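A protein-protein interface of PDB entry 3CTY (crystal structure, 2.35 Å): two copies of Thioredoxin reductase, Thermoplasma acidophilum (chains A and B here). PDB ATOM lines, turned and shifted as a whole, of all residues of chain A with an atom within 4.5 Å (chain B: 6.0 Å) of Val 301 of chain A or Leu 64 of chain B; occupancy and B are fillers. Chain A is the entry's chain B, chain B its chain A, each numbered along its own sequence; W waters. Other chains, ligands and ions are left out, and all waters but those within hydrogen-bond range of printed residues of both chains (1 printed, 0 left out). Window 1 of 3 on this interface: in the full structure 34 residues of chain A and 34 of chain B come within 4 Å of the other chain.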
ATOM      1  N   ALA A  26      13.193 -12.139 -13.363  1.00  0.00           N
ATOM      2  CA  ALA A  26      12.607 -13.487 -13.465  1.00  0.00           C
ATOM      3  C   ALA A  26      12.131 -13.840 -14.872  1.00  0.00           C
ATOM      4  O   ALA A  26      12.518 -14.867 -15.406  1.00  0.00           O
ATOM      5  CB  ALA A  26      11.460 -13.643 -12.483  1.00  0.00           C
ATOM      6  N   PHE A  29      15.191 -13.887 -17.470  1.00  0.00           N
ATOM      7  CA  PHE A  29      16.046 -15.041 -17.231  1.00  0.00           C
ATOM      8  C   PHE A  29      15.449 -16.330 -17.800  1.00  0.00           C
ATOM      9  O   PHE A  29      16.135 -17.101 -18.488  1.00  0.00           O
ATOM     10  CB  PHE A  29      16.297 -15.219 -15.735  1.00  0.00           C
ATOM     11  CG  PHE A  29      17.178 -14.162 -15.126  1.00  0.00           C
ATOM     12  CD1 PHE A  29      18.390 -13.815 -15.719  1.00  0.00           C
ATOM     13  CD2 PHE A  29      16.814 -13.537 -13.936  1.00  0.00           C
ATOM     14  CE1 PHE A  29      19.224 -12.866 -15.139  1.00  0.00           C
ATOM     15  CE2 PHE A  29      17.644 -12.585 -13.342  1.00  0.00           C
ATOM     16  CZ  PHE A  29      18.850 -12.249 -13.945  1.00  0.00           C
ATOM     17  N   SER A  30      14.171 -16.567 -17.509  1.00  0.00           N
ATOM     18  CA  SER A  30      13.500 -17.760 -18.010  1.00  0.00           C
ATOM     19  C   SER A  30      13.540 -17.731 -19.542  1.00  0.00           C
ATOM     20  O   SER A  30      13.942 -18.694 -20.186  1.00  0.00           O
ATOM     21  CB  SER A  30      12.052 -17.801 -17.513  1.00  0.00           C
ATOM     22  OG  SER A  30      11.400 -18.975 -17.960  1.00  0.00           O
ATOM     23  N   VAL A  33      17.048 -18.719 -20.937  1.00  0.00           N
ATOM     24  CA  VAL A  33      17.326 -20.144 -20.926  1.00  0.00           C
ATOM     25  C   VAL A  33      16.611 -20.815 -22.110  1.00  0.00           C
ATOM     26  O   VAL A  33      17.233 -21.515 -22.908  1.00  0.00           O
ATOM     27  CB  VAL A  33      16.840 -20.787 -19.603  1.00  0.00           C
ATOM     28  CG1 VAL A  33      16.975 -22.289 -19.678  1.00  0.00           C
ATOM     29  CG2 VAL A  33      17.661 -20.246 -18.434  1.00  0.00           C
ATOM     30  N   TYR A  63       6.815 -19.765  -4.853  1.00  0.00           N
ATOM     31  CA  TYR A  63       7.402 -20.134  -6.139  1.00  0.00           C
ATOM     32  C   TYR A  63       7.694 -21.628  -6.005  1.00  0.00           C
ATOM     33  O   TYR A  63       8.656 -22.015  -5.349  1.00  0.00           O
ATOM     34  CB  TYR A  63       8.697 -19.376  -6.389  1.00  0.00           C
ATOM     35  CG  TYR A  63       9.371 -19.779  -7.680  1.00  0.00           C
ATOM     36  CD1 TYR A  63       8.714 -19.648  -8.899  1.00  0.00           C
ATOM     37  CD2 TYR A  63      10.660 -20.317  -7.678  1.00  0.00           C
ATOM     38  CE1 TYR A  63       9.321 -20.041 -10.090  1.00  0.00           C
ATOM     39  CE2 TYR A  63      11.275 -20.720  -8.869  1.00  0.00           C
ATOM     40  CZ  TYR A  63      10.601 -20.579 -10.069  1.00  0.00           C
ATOM     41  OH  TYR A  63      11.203 -20.971 -11.244  1.00  0.00           O
ATOM     42  N   PHE A  78      18.677 -17.580 -10.071  1.00  0.00           N
ATOM     43  CA  PHE A  78      18.117 -17.322 -11.385  1.00  0.00           C
ATOM     44  C   PHE A  78      19.223 -16.838 -12.316  1.00  0.00           C
ATOM     45  O   PHE A  78      19.394 -17.355 -13.429  1.00  0.00           O
ATOM     46  CB  PHE A  78      17.020 -16.248 -11.298  1.00  0.00           C
ATOM     47  CG  PHE A  78      15.713 -16.737 -10.725  1.00  0.00           C
ATOM     48  CD1 PHE A  78      15.531 -18.078 -10.379  1.00  0.00           C
ATOM     49  CD2 PHE A  78      14.641 -15.865 -10.580  1.00  0.00           C
ATOM     50  CE1 PHE A  78      14.297 -18.536  -9.904  1.00  0.00           C
ATOM     51  CE2 PHE A  78      13.404 -16.312 -10.105  1.00  0.00           C
ATOM     52  CZ  PHE A  78      13.231 -17.646  -9.769  1.00  0.00           C
ATOM     53  N   HIS A  81      21.690 -19.437 -13.248  1.00  0.00           N
ATOM     54  CA  HIS A  81      21.089 -20.383 -14.165  1.00  0.00           C
ATOM     55  C   HIS A  81      21.152 -19.782 -15.581  1.00  0.00           C
ATOM     56  O   HIS A  81      21.643 -20.401 -16.524  1.00  0.00           O
ATOM     57  CB  HIS A  81      19.633 -20.638 -13.739  1.00  0.00           C
ATOM     58  CG  HIS A  81      18.974 -21.787 -14.443  1.00  0.00           C
ATOM     59  ND1 HIS A  81      17.735 -22.272 -14.074  1.00  0.00           N
ATOM     60  CD2 HIS A  81      19.375 -22.542 -15.494  1.00  0.00           C
ATOM     61  CE1 HIS A  81      17.403 -23.274 -14.868  1.00  0.00           C
ATOM     62  NE2 HIS A  81      18.382 -23.455 -15.737  1.00  0.00           N
ATOM     63  N   ILE A 297       6.527 -13.994  -9.354  1.00  0.00           N
ATOM     64  CA  ILE A 297       7.712 -14.578  -9.947  1.00  0.00           C
ATOM     65  C   ILE A 297       7.289 -15.761 -10.839  1.00  0.00           C
ATOM     66  O   ILE A 297       7.677 -15.850 -12.018  1.00  0.00           O
ATOM     67  CB  ILE A 297       8.659 -15.071  -8.853  1.00  0.00           C
ATOM     68  CG1 ILE A 297       9.128 -13.888  -7.998  1.00  0.00           C
ATOM     69  CG2 ILE A 297       9.834 -15.806  -9.472  1.00  0.00           C
ATOM     70  CD1 ILE A 297       9.775 -14.311  -6.707  1.00  0.00           C
ATOM     71  N   ALA A 298       6.481 -16.648 -10.265  1.00  0.00           N
ATOM     72  CA  ALA A 298       5.982 -17.845 -10.954  1.00  0.00           C
ATOM     73  C   ALA A 298       5.413 -17.579 -12.333  1.00  0.00           C
ATOM     74  O   ALA A 298       5.821 -18.224 -13.312  1.00  0.00           O
ATOM     75  CB  ALA A 298       4.910 -18.548 -10.109  1.00  0.00           C
ATOM     76  N   SER A 299       4.460 -16.654 -12.416  1.00  0.00           N
ATOM     77  CA  SER A 299       3.838 -16.367 -13.706  1.00  0.00           C
ATOM     78  C   SER A 299       4.827 -15.671 -14.624  1.00  0.00           C
ATOM     79  O   SER A 299       4.755 -15.802 -15.850  1.00  0.00           O
ATOM     80  CB  SER A 299       2.575 -15.512 -13.541  1.00  0.00           C
ATOM     81  OG  SER A 299       2.870 -14.220 -13.041  1.00  0.00           O
ATOM     82  N   ALA A 300       5.761 -14.939 -14.027  1.00  0.00           N
ATOM     83  CA  ALA A 300       6.769 -14.246 -14.803  1.00  0.00           C
ATOM     84  C   ALA A 300       7.639 -15.292 -15.485  1.00  0.00           C
ATOM     85  O   ALA A 300       7.900 -15.201 -16.681  1.00  0.00           O
ATOM     86  CB  ALA A 300       7.613 -13.367 -13.908  1.00  0.00           C
ATOM     87  N   VAL A 301       8.070 -16.291 -14.718  1.00  0.00           N
ATOM     88  CA  VAL A 301       8.922 -17.351 -15.246  1.00  0.00           C
ATOM     89  C   VAL A 301       8.168 -18.072 -16.345  1.00  0.00           C
ATOM     90  O   VAL A 301       8.712 -18.312 -17.445  1.00  0.00           O
ATOM     91  CB  VAL A 301       9.325 -18.351 -14.138  1.00  0.00           C
ATOM     92  CG1 VAL A 301       9.991 -19.560 -14.742  1.00  0.00           C
ATOM     93  CG2 VAL A 301      10.284 -17.683 -13.160  1.00  0.00           C
ATOM     94  N   GLY A 302       6.904 -18.377 -16.046  1.00  0.00           N
ATOM     95  CA  GLY A 302       6.052 -19.069 -16.982  1.00  0.00           C
ATOM     96  C   GLY A 302       5.931 -18.339 -18.300  1.00  0.00           C
ATOM     97  O   GLY A 302       6.203 -18.922 -19.344  1.00  0.00           O
ATOM     98  N   ASP A 303       5.536 -17.069 -18.263  1.00  0.00           N
ATOM     99  CA  ASP A 303       5.392 -16.303 -19.501  1.00  0.00           C
ATOM    100  C   ASP A 303       6.734 -16.094 -20.219  1.00  0.00           C
ATOM    101  O   ASP A 303       6.791 -16.053 -21.466  1.00  0.00           O
ATOM    102  CB  ASP A 303       4.684 -14.967 -19.218  1.00  0.00           C
ATOM    103  CG  ASP A 303       3.217 -15.167 -18.773  1.00  0.00           C
ATOM    104  OD1 ASP A 303       2.752 -16.336 -18.736  1.00  0.00           O
ATOM    105  OD2 ASP A 303       2.528 -14.169 -18.460  1.00  0.00           O
ATOM    106  N   GLY A 304       7.809 -15.986 -19.442  1.00  0.00           N
ATOM    107  CA  GLY A 304       9.122 -15.817 -20.040  1.00  0.00           C
ATOM    108  C   GLY A 304       9.404 -17.052 -20.889  1.00  0.00           C
ATOM    109  O   GLY A 304       9.962 -16.968 -21.996  1.00  0.00           O
ATOM    110  N   CYS A 305       8.993 -18.199 -20.357  1.00  0.00           N
ATOM    111  CA  CYS A 305       9.154 -19.487 -21.028  1.00  0.00           C
ATOM    112  C   CYS A 305       8.357 -19.456 -22.330  1.00  0.00           C
ATOM    113  O   CYS A 305       8.893 -19.754 -23.397  1.00  0.00           O
ATOM    114  CB  CYS A 305       8.648 -20.617 -20.123  1.00  0.00           C
ATOM    115  SG  CYS A 305       8.287 -22.161 -20.983  1.00  0.00           S
ATOM    116  N   ASN B  62      15.513 -26.622 -17.528  1.00  0.00           N
ATOM    117  CA  ASN B  62      14.921 -25.345 -17.908  1.00  0.00           C
ATOM    118  C   ASN B  62      13.804 -24.841 -17.001  1.00  0.00           C
ATOM    119  O   ASN B  62      12.900 -24.150 -17.455  1.00  0.00           O
ATOM    120  CB  ASN B  62      14.404 -25.411 -19.343  1.00  0.00           C
ATOM    121  CG  ASN B  62      13.524 -26.608 -19.574  1.00  0.00           C
ATOM    122  OD1 ASN B  62      12.910 -27.131 -18.637  1.00  0.00           O
ATOM    123  ND2 ASN B  62      13.447 -27.051 -20.822  1.00  0.00           N
ATOM    124  N   TYR B  63      13.835 -25.230 -15.737  1.00  0.00           N
ATOM    125  CA  TYR B  63      12.870 -24.720 -14.770  1.00  0.00           C
ATOM    126  C   TYR B  63      13.725 -23.721 -13.961  1.00  0.00           C
ATOM    127  O   TYR B  63      14.572 -24.124 -13.169  1.00  0.00           O
ATOM    128  CB  TYR B  63      12.346 -25.827 -13.866  1.00  0.00           C
ATOM    129  CG  TYR B  63      11.360 -25.295 -12.862  1.00  0.00           C
ATOM    130  CD1 TYR B  63      10.179 -24.683 -13.278  1.00  0.00           C
ATOM    131  CD2 TYR B  63      11.631 -25.347 -11.494  1.00  0.00           C
ATOM    132  CE1 TYR B  63       9.291 -24.126 -12.358  1.00  0.00           C
ATOM    133  CE2 TYR B  63      10.749 -24.795 -10.558  1.00  0.00           C
ATOM    134  CZ  TYR B  63       9.581 -24.183 -11.000  1.00  0.00           C
ATOM    135  OH  TYR B  63       8.711 -23.622 -10.090  1.00  0.00           O
ATOM    136  N   LEU B  64      13.506 -22.429 -14.178  1.00  0.00           N
ATOM    137  CA  LEU B  64      14.309 -21.393 -13.529  1.00  0.00           C
ATOM    138  C   LEU B  64      14.635 -21.595 -12.052  1.00  0.00           C
ATOM    139  O   LEU B  64      13.747 -21.752 -11.220  1.00  0.00           O
ATOM    140  CB  LEU B  64      13.665 -20.027 -13.730  1.00  0.00           C
ATOM    141  CG  LEU B  64      14.496 -18.927 -14.404  1.00  0.00           C
ATOM    142  CD1 LEU B  64      14.305 -17.621 -13.635  1.00  0.00           C
ATOM    143  CD2 LEU B  64      15.975 -19.310 -14.463  1.00  0.00           C
ATOM    144  N   GLY B  65      15.929 -21.592 -11.738  1.00  0.00           N
ATOM    145  CA  GLY B  65      16.355 -21.780 -10.363  1.00  0.00           C
ATOM    146  C   GLY B  65      17.067 -23.103 -10.132  1.00  0.00           C
ATOM    147  O   GLY B  65      17.836 -23.237  -9.172  1.00  0.00           O
ATOM    148  N   PHE B  66      16.790 -24.084 -10.993  1.00  0.00           N
ATOM    149  CA  PHE B  66      17.428 -25.400 -10.916  1.00  0.00           C
ATOM    150  C   PHE B  66      18.254 -25.587 -12.186  1.00  0.00           C
ATOM    151  O   PHE B  66      17.701 -25.722 -13.281  1.00  0.00           O
ATOM    152  CB  PHE B  66      16.384 -26.512 -10.834  1.00  0.00           C
ATOM    153  CG  PHE B  66      15.538 -26.461  -9.604  1.00  0.00           C
ATOM    154  CD1 PHE B  66      14.356 -25.727  -9.587  1.00  0.00           C
ATOM    155  CD2 PHE B  66      15.908 -27.163  -8.462  1.00  0.00           C
ATOM    156  CE1 PHE B  66      13.550 -25.697  -8.452  1.00  0.00           C
ATOM    157  CE2 PHE B  66      15.105 -27.139  -7.316  1.00  0.00           C
ATOM    158  CZ  PHE B  66      13.927 -26.409  -7.313  1.00  0.00           C
ATOM    159  N   ALA B 298       7.732 -24.971 -16.294  1.00  0.00           N
ATOM    160  CA  ALA B 298       7.688 -23.537 -16.007  1.00  0.00           C
ATOM    161  C   ALA B 298       6.336 -22.878 -16.325  1.00  0.00           C
ATOM    162  O   ALA B 298       5.819 -22.097 -15.514  1.00  0.00           O
ATOM    163  CB  ALA B 298       8.798 -22.818 -16.757  1.00  0.00           C
ATOM    164  N   SER B 299       5.763 -23.184 -17.487  1.00  0.00           N
ATOM    165  CA  SER B 299       4.484 -22.577 -17.862  1.00  0.00           C
ATOM    166  C   SER B 299       3.338 -23.123 -17.045  1.00  0.00           C
ATOM    167  O   SER B 299       2.393 -22.402 -16.746  1.00  0.00           O
ATOM    168  CB  SER B 299       4.182 -22.768 -19.354  1.00  0.00           C
ATOM    169  OG  SER B 299       4.108 -24.142 -19.705  1.00  0.00           O
HETATM  170  O   HOH W   1      12.255 -21.552 -16.774  1.00  0.00           O
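Water W1 lies within hydrogen-bond range of O of Asn 62 of chain B, OG of Ser 30 of chain A and N of Leu 64 of chain B.
Tyr 63 of chain B touches its own counterpart, Tyr 63 of chain A.
Positions printed for both chains: 63, 298 and 299.
Of the 14 pairs that touch across the chains among the printed residues, 1 has its exchanged pair printed and touching as well.
Among the printed residues, merely in contact across the chains: Ala 26 of chain A with Leu 64 of chain B, Phe 29 of chain A with Leu 64 of chain B, Ser 30 of chain A with Leu 64 of chain B, Tyr 63 of chain A with Tyr 63 of chain B, Phe 78 of chain A with Leu 64 of chain B, Phe 78 of chain A with Gly 65 of chain B, His 81 of chain A with Tyr 63 of chain B, His 81 of chain A with Leu 64 of chain B, Val 301 of chain A with Leu 64 of chain B, Gly 302 of chain A with Ala 298 of chain B and Gly 302 of chain A with Ser 299 of chain B.
Printed residues of chain B within 4 Å of Phe 29 of chain A: Leu 64 (3.8 Å).
Printed residues of chain B within 4 Å of Ser 30 of chain A: Leu 64.
Of the printed residues of chain B, Val 301 of chain A touches Leu 64.
Of the printed residues of chain B, Gly 302 of chain A touches Ala 298 and Ser 299.
Of the printed residues of chain A, Phe 66 of chain B touches His 81 (2.9 Å).
Printed residues of chain A within 4 Å of Ser 299 of chain B: Gly 302 (3.9 Å).
The nearest residue of chain A that does not touch Leu 64 of chain B is Val 33 of chain A (4.4 Å).
The nearest printed residue of chain B that does not touch Ser 30 of chain A is Ala 298 of chain B (4.8 Å).
Of the 7 printed residues of chain B, 6 touch a printed residue of chain A.
Among the printed residues, 14 pairs touch across the chains.
Among the printed residues, no Asp or Glu carboxylate lies within 4 Å of a Lys or Arg side-chain nitrogen of the other chain.
The side-chain hydroxyl (OG) of Ser 30 of chain A sits at hydrogen-bond distance from the backbone carbonyl oxygen (O) of Val 301 of chain A (2.8 Å).
The backbone NH of Cys 305 of chain A sits at hydrogen-bond distance from the side-chain hydroxyl of Ser 30 of chain A, 3.5 Å away.
N of Gly 65 of chain B is in hydrogen-bond range of ND1 of His 81 of chain A, 3.0 Å away.
The side-chain hydroxyl (OH) of Tyr 63 of chain A sits at hydrogen-bond distance from the backbone carbonyl oxygen (O) of Leu 64 of chain B (2.7 Å).
A ring nitrogen (NE2) of His 81 of chain A lies close to the backbone carbonyl oxygen (O) of Phe 66 of chain B, at 3.4 Å.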
